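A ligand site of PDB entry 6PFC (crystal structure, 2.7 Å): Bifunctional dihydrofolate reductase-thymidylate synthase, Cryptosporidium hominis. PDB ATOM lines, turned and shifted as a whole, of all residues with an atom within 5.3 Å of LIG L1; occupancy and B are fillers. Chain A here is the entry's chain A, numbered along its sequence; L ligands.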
ATOM      1  N   ARG A 257     -10.421   1.012 -28.442  1.00  0.00           N
ATOM      2  CA  ARG A 257      -9.813   2.028 -27.588  1.00  0.00           C
ATOM      3  C   ARG A 257      -9.514   1.515 -26.181  1.00  0.00           C
ATOM      4  O   ARG A 257      -8.683   2.109 -25.492  1.00  0.00           O
ATOM      5  CB  ARG A 257     -10.737   3.246 -27.506  1.00  0.00           C
ATOM      6  CG  ARG A 257     -12.133   2.927 -26.989  1.00  0.00           C
ATOM      7  CD  ARG A 257     -12.937   4.183 -26.730  1.00  0.00           C
ATOM      8  NE  ARG A 257     -14.232   3.883 -26.126  1.00  0.00           N
ATOM      9  CZ  ARG A 257     -14.413   3.713 -24.819  1.00  0.00           C
ATOM     10  NH1 ARG A 257     -13.393   3.808 -23.987  1.00  0.00           N
ATOM     11  NH2 ARG A 257     -15.626   3.431 -24.353  1.00  0.00           N
ATOM     12  N   LYS A 284     -31.025 -13.998 -17.553  1.00  0.00           N
ATOM     13  CA  LYS A 284     -30.108 -13.310 -16.663  1.00  0.00           C
ATOM     14  C   LYS A 284     -30.873 -12.238 -15.917  1.00  0.00           C
ATOM     15  O   LYS A 284     -31.672 -11.513 -16.509  1.00  0.00           O
ATOM     16  CB  LYS A 284     -28.943 -12.688 -17.444  1.00  0.00           C
ATOM     17  CG  LYS A 284     -27.988 -11.850 -16.611  1.00  0.00           C
ATOM     18  CD  LYS A 284     -26.956 -11.154 -17.489  1.00  0.00           C
ATOM     19  CE  LYS A 284     -27.606 -10.127 -18.402  1.00  0.00           C
ATOM     20  NZ  LYS A 284     -26.592  -9.396 -19.219  1.00  0.00           N
ATOM     21  N   LYS A 285     -30.641 -12.134 -14.611  1.00  0.00           N
ATOM     22  CA  LYS A 285     -31.296 -11.114 -13.796  1.00  0.00           C
ATOM     23  C   LYS A 285     -30.754  -9.744 -14.168  1.00  0.00           C
ATOM     24  O   LYS A 285     -29.575  -9.456 -13.962  1.00  0.00           O
ATOM     25  CB  LYS A 285     -31.091 -11.407 -12.317  1.00  0.00           C
ATOM     26  CG  LYS A 285     -31.852 -10.469 -11.384  1.00  0.00           C
ATOM     27  CD  LYS A 285     -31.681 -10.864  -9.933  1.00  0.00           C
ATOM     28  CE  LYS A 285     -32.392  -9.883  -9.011  1.00  0.00           C
ATOM     29  NZ  LYS A 285     -32.265 -10.263  -7.579  1.00  0.00           N
ATOM     30  N   ALA A 287     -30.715  -5.626 -13.832  1.00  0.00           N
ATOM     31  CA  ALA A 287     -30.983  -4.564 -12.880  1.00  0.00           C
ATOM     32  C   ALA A 287     -31.948  -3.538 -13.453  1.00  0.00           C
ATOM     33  O   ALA A 287     -31.523  -2.523 -14.005  1.00  0.00           O
ATOM     34  CB  ALA A 287     -29.681  -3.889 -12.451  1.00  0.00           C
ATOM     35  N   SER A 290     -31.711   0.234 -12.031  1.00  0.00           N
ATOM     36  CA  SER A 290     -30.648   1.058 -12.597  1.00  0.00           C
ATOM     37  C   SER A 290     -30.980   1.517 -14.006  1.00  0.00           C
ATOM     38  O   SER A 290     -30.605   2.619 -14.407  1.00  0.00           O
ATOM     39  CB  SER A 290     -29.310   0.304 -12.578  1.00  0.00           C
ATOM     40  OG  SER A 290     -28.950  -0.091 -11.260  1.00  0.00           O
ATOM     41  N   GLU A 294     -31.367   5.561 -15.033  1.00  0.00           N
ATOM     42  CA  GLU A 294     -30.603   6.168 -16.112  1.00  0.00           C
ATOM     43  C   GLU A 294     -31.511   6.840 -17.134  1.00  0.00           C
ATOM     44  O   GLU A 294     -31.188   7.908 -17.661  1.00  0.00           O
ATOM     45  CB  GLU A 294     -29.718   5.112 -16.781  1.00  0.00           C
ATOM     46  CG  GLU A 294     -28.840   5.635 -17.901  1.00  0.00           C
ATOM     47  CD  GLU A 294     -28.333   4.525 -18.814  1.00  0.00           C
ATOM     48  OE1 GLU A 294     -29.098   3.572 -19.062  1.00  0.00           O
ATOM     49  OE2 GLU A 294     -27.178   4.613 -19.289  1.00  0.00           O
ATOM     50  N   TYR A 314     -24.075   2.939 -10.433  1.00  0.00           N
ATOM     51  CA  TYR A 314     -22.658   3.162 -10.711  1.00  0.00           C
ATOM     52  C   TYR A 314     -22.287   2.750 -12.136  1.00  0.00           C
ATOM     53  O   TYR A 314     -21.142   2.400 -12.414  1.00  0.00           O
ATOM     54  CB  TYR A 314     -21.796   2.419  -9.699  1.00  0.00           C
ATOM     55  CG  TYR A 314     -22.302   2.518  -8.280  1.00  0.00           C
ATOM     56  CD1 TYR A 314     -22.023   3.633  -7.494  1.00  0.00           C
ATOM     57  CD2 TYR A 314     -23.051   1.489  -7.720  1.00  0.00           C
ATOM     58  CE1 TYR A 314     -22.487   3.715  -6.193  1.00  0.00           C
ATOM     59  CE2 TYR A 314     -23.516   1.572  -6.420  1.00  0.00           C
ATOM     60  CZ  TYR A 314     -23.227   2.689  -5.663  1.00  0.00           C
ATOM     61  OH  TYR A 314     -23.696   2.784  -4.367  1.00  0.00           O
ATOM     62  N   ILE A 315     -23.253   2.776 -13.063  1.00  0.00           N
ATOM     63  CA  ILE A 315     -22.976   2.354 -14.421  1.00  0.00           C
ATOM     64  C   ILE A 315     -22.158   3.385 -15.179  1.00  0.00           C
ATOM     65  O   ILE A 315     -21.496   3.053 -16.175  1.00  0.00           O
ATOM     66  CB  ILE A 315     -24.275   2.030 -15.177  1.00  0.00           C
ATOM     67  CG1 ILE A 315     -25.147   3.287 -15.304  1.00  0.00           C
ATOM     68  CG2 ILE A 315     -25.040   0.911 -14.469  1.00  0.00           C
ATOM     69  CD1 ILE A 315     -26.408   3.069 -16.106  1.00  0.00           C
ATOM     70  N   TRP A 316     -22.166   4.644 -14.740  1.00  0.00           N
ATOM     71  CA  TRP A 316     -21.390   5.712 -15.367  1.00  0.00           C
ATOM     72  C   TRP A 316     -20.184   6.116 -14.528  1.00  0.00           C
ATOM     73  O   TRP A 316     -19.606   7.175 -14.766  1.00  0.00           O
ATOM     74  CB  TRP A 316     -22.283   6.920 -15.634  1.00  0.00           C
ATOM     75  CG  TRP A 316     -23.196   6.752 -16.812  1.00  0.00           C
ATOM     76  CD1 TRP A 316     -24.510   6.365 -16.783  1.00  0.00           C
ATOM     77  CD2 TRP A 316     -22.870   6.972 -18.184  1.00  0.00           C
ATOM     78  NE1 TRP A 316     -25.007   6.334 -18.061  1.00  0.00           N
ATOM     79  CE2 TRP A 316     -24.030   6.707 -18.937  1.00  0.00           C
ATOM     80  CE3 TRP A 316     -21.716   7.385 -18.853  1.00  0.00           C
ATOM     81  CZ2 TRP A 316     -24.062   6.812 -20.328  1.00  0.00           C
ATOM     82  CZ3 TRP A 316     -21.744   7.496 -20.229  1.00  0.00           C
ATOM     83  CH2 TRP A 316     -22.917   7.217 -20.953  1.00  0.00           C
ATOM     84  N   ASN A 319     -16.640   5.600 -16.815  1.00  0.00           N
ATOM     85  CA  ASN A 319     -16.452   6.632 -17.816  1.00  0.00           C
ATOM     86  C   ASN A 319     -16.532   8.046 -17.228  1.00  0.00           C
ATOM     87  O   ASN A 319     -16.554   9.010 -18.000  1.00  0.00           O
ATOM     88  CB  ASN A 319     -17.485   6.472 -18.933  1.00  0.00           C
ATOM     89  CG  ASN A 319     -17.463   5.088 -19.550  1.00  0.00           C
ATOM     90  OD1 ASN A 319     -18.229   4.212 -19.149  1.00  0.00           O
ATOM     91  ND2 ASN A 319     -16.587   4.876 -20.522  1.00  0.00           N
ATOM     92  N   LEU A 399     -18.100  10.446 -23.528  1.00  0.00           N
ATOM     93  CA  LEU A 399     -18.293   9.270 -24.376  1.00  0.00           C
ATOM     94  C   LEU A 399     -19.322   9.606 -25.456  1.00  0.00           C
ATOM     95  O   LEU A 399     -20.442  10.035 -25.133  1.00  0.00           O
ATOM     96  CB  LEU A 399     -18.750   8.078 -23.540  1.00  0.00           C
ATOM     97  CG  LEU A 399     -18.702   6.702 -24.224  1.00  0.00           C
ATOM     98  CD1 LEU A 399     -17.274   6.340 -24.591  1.00  0.00           C
ATOM     99  CD2 LEU A 399     -19.318   5.643 -23.330  1.00  0.00           C
ATOM    100  N   ASP A 426     -22.280  -3.164 -26.771  1.00  0.00           N
ATOM    101  CA  ASP A 426     -21.713  -4.122 -25.832  1.00  0.00           C
ATOM    102  C   ASP A 426     -22.807  -5.151 -25.515  1.00  0.00           C
ATOM    103  O   ASP A 426     -23.703  -4.887 -24.718  1.00  0.00           O
ATOM    104  CB  ASP A 426     -21.220  -3.423 -24.571  1.00  0.00           C
ATOM    105  CG  ASP A 426     -20.500  -4.360 -23.617  1.00  0.00           C
ATOM    106  OD1 ASP A 426     -20.452  -5.582 -23.877  1.00  0.00           O
ATOM    107  OD2 ASP A 426     -19.975  -3.862 -22.598  1.00  0.00           O
ATOM    108  N   GLY A 428     -22.720  -7.850 -23.853  1.00  0.00           N
ATOM    109  CA  GLY A 428     -22.705  -8.404 -22.508  1.00  0.00           C
ATOM    110  C   GLY A 428     -23.381  -7.516 -21.488  1.00  0.00           C
ATOM    111  O   GLY A 428     -24.079  -8.006 -20.594  1.00  0.00           O
ATOM    112  N   LEU A 429     -23.180  -6.197 -21.602  1.00  0.00           N
ATOM    113  CA  LEU A 429     -23.688  -5.250 -20.618  1.00  0.00           C
ATOM    114  C   LEU A 429     -24.635  -4.223 -21.215  1.00  0.00           C
ATOM    115  O   LEU A 429     -25.757  -4.052 -20.712  1.00  0.00           O
ATOM    116  CB  LEU A 429     -22.516  -4.544 -19.924  1.00  0.00           C
ATOM    117  CG  LEU A 429     -21.587  -5.433 -19.102  1.00  0.00           C
ATOM    118  CD1 LEU A 429     -20.487  -4.614 -18.459  1.00  0.00           C
ATOM    119  CD2 LEU A 429     -22.371  -6.207 -18.052  1.00  0.00           C
ATOM    120  N   GLY A 430     -24.214  -3.523 -22.273  1.00  0.00           N
ATOM    121  CA  GLY A 430     -25.023  -2.433 -22.791  1.00  0.00           C
ATOM    122  C   GLY A 430     -26.319  -2.878 -23.423  1.00  0.00           C
ATOM    123  O   GLY A 430     -27.368  -2.264 -23.219  1.00  0.00           O
ATOM    124  N   PHE A 433     -29.441  -3.453 -21.266  1.00  0.00           N
ATOM    125  CA  PHE A 433     -29.903  -2.163 -20.777  1.00  0.00           C
ATOM    126  C   PHE A 433     -30.622  -1.376 -21.869  1.00  0.00           C
ATOM    127  O   PHE A 433     -31.680  -0.800 -21.622  1.00  0.00           O
ATOM    128  CB  PHE A 433     -28.732  -1.355 -20.219  1.00  0.00           C
ATOM    129  CG  PHE A 433     -28.420  -1.637 -18.773  1.00  0.00           C
ATOM    130  CD1 PHE A 433     -28.274  -2.945 -18.326  1.00  0.00           C
ATOM    131  CD2 PHE A 433     -28.272  -0.608 -17.873  1.00  0.00           C
ATOM    132  CE1 PHE A 433     -27.982  -3.216 -17.006  1.00  0.00           C
ATOM    133  CE2 PHE A 433     -27.984  -0.870 -16.544  1.00  0.00           C
ATOM    134  CZ  PHE A 433     -27.839  -2.175 -16.111  1.00  0.00           C
ATOM    135  N   TYR A 466     -17.035  -8.503 -25.664  1.00  0.00           N
ATOM    136  CA  TYR A 466     -15.729  -8.374 -25.043  1.00  0.00           C
ATOM    137  C   TYR A 466     -15.200  -9.734 -24.612  1.00  0.00           C
ATOM    138  O   TYR A 466     -15.945 -10.582 -24.120  1.00  0.00           O
ATOM    139  CB  TYR A 466     -15.803  -7.423 -23.849  1.00  0.00           C
ATOM    140  CG  TYR A 466     -15.922  -5.963 -24.248  1.00  0.00           C
ATOM    141  CD1 TYR A 466     -17.155  -5.389 -24.492  1.00  0.00           C
ATOM    142  CD2 TYR A 466     -14.787  -5.179 -24.402  1.00  0.00           C
ATOM    143  CE1 TYR A 466     -17.267  -4.053 -24.864  1.00  0.00           C
ATOM    144  CE2 TYR A 466     -14.878  -3.849 -24.770  1.00  0.00           C
ATOM    145  CZ  TYR A 466     -16.114  -3.297 -25.004  1.00  0.00           C
ATOM    146  OH  TYR A 466     -16.215  -1.974 -25.380  1.00  0.00           O
ATOM    147  N   THR A 514     -28.210 -13.817 -11.581  1.00  0.00           N
ATOM    148  CA  THR A 514     -27.430 -12.778 -12.230  1.00  0.00           C
ATOM    149  C   THR A 514     -26.028 -13.272 -12.581  1.00  0.00           C
ATOM    150  O   THR A 514     -25.486 -14.175 -11.933  1.00  0.00           O
ATOM    151  CB  THR A 514     -27.348 -11.540 -11.338  1.00  0.00           C
ATOM    152  OG1 THR A 514     -26.361 -10.632 -11.861  1.00  0.00           O
ATOM    153  CG2 THR A 514     -26.961 -11.932  -9.913  1.00  0.00           C
ATOM    154  N   ILE A 515     -25.448 -12.672 -13.609  1.00  0.00           N
ATOM    155  CA  ILE A 515     -24.135 -13.037 -14.124  1.00  0.00           C
ATOM    156  C   ILE A 515     -23.247 -11.799 -14.080  1.00  0.00           C
ATOM    157  O   ILE A 515     -23.552 -10.789 -14.724  1.00  0.00           O
ATOM    158  CB  ILE A 515     -24.210 -13.609 -15.546  1.00  0.00           C
ATOM    159  CG1 ILE A 515     -25.194 -14.779 -15.598  1.00  0.00           C
ATOM    160  CG2 ILE A 515     -22.838 -14.053 -16.006  1.00  0.00           C
ATOM    161  CD1 ILE A 515     -25.371 -15.375 -16.984  1.00  0.00           C
ATOM    162  N   MET A 517     -20.255  -9.373 -14.896  1.00  0.00           N
ATOM    163  CA  MET A 517     -19.398  -9.062 -16.035  1.00  0.00           C
ATOM    164  C   MET A 517     -18.784  -7.693 -15.830  1.00  0.00           C
ATOM    165  O   MET A 517     -19.489  -6.733 -15.478  1.00  0.00           O
ATOM    166  CB  MET A 517     -20.190  -9.075 -17.344  1.00  0.00           C
ATOM    167  CG  MET A 517     -20.527 -10.445 -17.891  1.00  0.00           C
ATOM    168  SD  MET A 517     -21.494 -10.319 -19.402  1.00  0.00           S
ATOM    169  CE  MET A 517     -23.104 -10.891 -18.875  1.00  0.00           C
ATOM    170  N   MET A 519     -17.065  -4.111 -16.798  1.00  0.00           N
ATOM    171  CA  MET A 519     -17.189  -3.115 -17.857  1.00  0.00           C
ATOM    172  C   MET A 519     -15.814  -2.648 -18.298  1.00  0.00           C
ATOM    173  O   MET A 519     -14.933  -2.412 -17.467  1.00  0.00           O
ATOM    174  CB  MET A 519     -18.029  -1.925 -17.388  1.00  0.00           C
ATOM    175  CG  MET A 519     -18.286  -0.879 -18.470  1.00  0.00           C
ATOM    176  SD  MET A 519     -18.704   0.742 -17.805  1.00  0.00           S
ATOM    177  CE  MET A 519     -17.203   1.131 -16.898  1.00  0.00           C
ATOM    178  N   ALA A 520     -15.641  -2.506 -19.612  1.00  0.00           N
ATOM    179  CA  ALA A 520     -14.393  -1.996 -20.159  1.00  0.00           C
ATOM    180  C   ALA A 520     -14.422  -0.472 -20.167  1.00  0.00           C
ATOM    181  O   ALA A 520     -15.314   0.144 -20.780  1.00  0.00           O
ATOM    182  CB  ALA A 520     -14.171  -2.530 -21.573  1.00  0.00           C
HETATM  183  O1  LIG L   1     -22.210  -0.918 -21.253  1.00  0.00           O
HETATM  184  C1  LIG L   1     -21.601   3.387 -20.380  1.00  0.00           C
HETATM  185  C2  LIG L   1     -23.634   1.834 -20.034  1.00  0.00           C
HETATM  186  C3  LIG L   1     -24.571  -0.292 -18.972  1.00  0.00           C
HETATM  187  C4  LIG L   1     -24.503  -1.327 -18.018  1.00  0.00           C
HETATM  188  C5  LIG L   1     -23.446  -1.377 -17.086  1.00  0.00           C
HETATM  189  C6  LIG L   1     -22.450  -0.380 -17.127  1.00  0.00           C
HETATM  190  C7  LIG L   1     -22.521   0.663 -18.071  1.00  0.00           C
HETATM  191  C8  LIG L   1     -23.344  -2.487 -16.059  1.00  0.00           C
HETATM  192  C9  LIG L   1     -24.665  -4.315 -15.003  1.00  0.00           C
HETATM  193  C10 LIG L   1     -24.608  -4.157 -13.588  1.00  0.00           C
HETATM  194  C11 LIG L   1     -25.079  -6.547 -13.306  1.00  0.00           C
HETATM  195  C12 LIG L   1     -24.923  -5.601 -15.539  1.00  0.00           C
HETATM  196  C13 LIG L   1     -24.965  -8.334 -16.476  1.00  0.00           C
HETATM  197  C14 LIG L   1     -24.349  -2.818 -12.900  1.00  0.00           C
HETATM  198  C15 LIG L   1     -25.583  -2.308 -12.163  1.00  0.00           C
HETATM  199  C16 LIG L   1     -20.108   1.971 -21.277  1.00  0.00           C
HETATM  200  C17 LIG L   1     -24.825  -5.282 -12.760  1.00  0.00           C
HETATM  201  C18 LIG L   1     -25.132  -6.730 -14.705  1.00  0.00           C
HETATM  202  C19 LIG L   1     -21.258   1.259 -21.046  1.00  0.00           C
HETATM  203  C20 LIG L   1     -21.245  -0.174 -21.410  1.00  0.00           C
HETATM  204  C21 LIG L   1     -18.969   0.205 -22.131  1.00  0.00           C
HETATM  205  C22 LIG L   1     -22.215   2.162 -20.470  1.00  0.00           C
HETATM  206  C23 LIG L   1     -23.579   0.714 -19.003  1.00  0.00           C
HETATM  207  N1  LIG L   1     -18.933   1.469 -21.821  1.00  0.00           N
HETATM  208  N2  LIG L   1     -20.086  -0.623 -21.940  1.00  0.00           N
HETATM  209  N3  LIG L   1     -20.320   3.268 -20.876  1.00  0.00           N
HETATM  210  N4  LIG L   1     -17.912  -0.485 -22.691  1.00  0.00           N
HETATM  211  N5  LIG L   1     -24.461  -3.208 -15.878  1.00  0.00           N
HETATM  212  O2  LIG L   1     -22.286  -2.671 -15.452  1.00  0.00           O
HETATM  213  O3  LIG L   1     -25.387  -8.001 -15.165  1.00  0.00           O
HETATM  214  O4  LIG L   1     -25.536  -1.708 -11.097  1.00  0.00           O
HETATM  215  O5  LIG L   1     -26.739  -2.612 -12.838  1.00  0.00           O
HETATM  216  N1  LG2 L   2     -22.235   0.807 -24.853  1.00  0.00           N
HETATM  217  C1  LG2 L   2     -23.385   0.245 -25.303  1.00  0.00           C
HETATM  218  N2  LG2 L   2     -24.578   0.790 -24.995  1.00  0.00           N
HETATM  219  C2  LG2 L   2     -24.671   1.913 -24.249  1.00  0.00           C
HETATM  220  C3  LG2 L   2     -23.480   2.513 -23.779  1.00  0.00           C
HETATM  221  C4  LG2 L   2     -22.295   1.939 -24.093  1.00  0.00           C
HETATM  222  O1  LG2 L   2     -23.403  -0.768 -25.981  1.00  0.00           O
HETATM  223  O2  LG2 L   2     -25.755   2.387 -23.986  1.00  0.00           O
HETATM  224  F1  LG2 L   2     -23.505   3.636 -23.019  1.00  0.00           F
HETATM  225  C5  LG2 L   2     -20.862   0.311 -25.113  1.00  0.00           C
HETATM  226  C6  LG2 L   2     -20.524   0.067 -26.597  1.00  0.00           C
HETATM  227  C7  LG2 L   2     -18.988   0.007 -26.518  1.00  0.00           C
HETATM  228  C8  LG2 L   2     -18.675   1.130 -25.507  1.00  0.00           C
HETATM  229  O3  LG2 L   2     -18.570  -1.241 -25.980  1.00  0.00           O
HETATM  230  O4  LG2 L   2     -19.905   1.339 -24.747  1.00  0.00           O
HETATM  231  C9  LG2 L   2     -18.237   2.425 -26.206  1.00  0.00           C
HETATM  232  O5  LG2 L   2     -18.310   2.260 -27.620  1.00  0.00           O
HETATM  233  P1  LG2 L   2     -17.059   3.034 -28.273  1.00  0.00           P
HETATM  234  O6  LG2 L   2     -17.013   2.742 -29.725  1.00  0.00           O
HETATM  235  O7  LG2 L   2     -15.699   2.515 -27.585  1.00  0.00           O
HETATM  236  O8  LG2 L   2     -17.203   4.612 -28.042  1.00  0.00           O
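The backbone NH (N) of Asp 426 is in hydrogen-bond range of an oxygen (O1) of LG2 L2 (2.8 Å).
N of Gly 430 sits at hydrogen-bond distance from O1 of LIG L1 (3.4 Å).
A nitrogen (N2) of LIG L1 sits at hydrogen-bond distance from the side-chain carboxylate (OD2) of Asp 426.
The backbone carbonyl oxygen (O) of Ala 520 is in hydrogen-bond range of a nitrogen (N4) of LIG L1 (3.3 Å).
The side-chain amide oxygen (OD1) of Asn 319 is in hydrogen-bond range of a nitrogen (N3) of LIG L1 (2.9 Å).
An oxygen (O7) of LG2 L2 lies within salt-bridge range of the guanidinium group (NE) of Arg 257 (2.5 Å).
An oxygen (O3) of LG2 L2 lies within hydrogen-bond range of the side-chain hydroxyl of Tyr 466 (2.5 Å).
A nitrogen (N4) of LIG L1 lies close to an oxygen (O4) of LG2 L2 (3.4 Å).
NZ of Lys 284 sits at hydrogen-bond distance from O of Gly 428, 3.2 Å away.
SD of Met 519 lies close to OD1 of Asn 319 (3.8 Å).
N of Gly 428 lies close to OD1 of Asp 426, at 3.2 Å.
The backbone carbonyl oxygen of Ile 515 sits close to an oxygen (O3) of LIG L1 (3.4 Å).
Residues that only touch LIG L1: Ile 315, Ala 287, Lys 284, Phe 433, Tyr 466, Leu 399, Leu 429, Ser 290, Met 519 and Met 517.
Hydrophobic or aromatic side chains within 4 Å of LIG L1: Ala 287, Ile 315, Leu 399, Leu 429, Phe 433, Met 517 and Met 519.
Of the 22 residues printed, 15 come within 4 Å of LIG L1.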
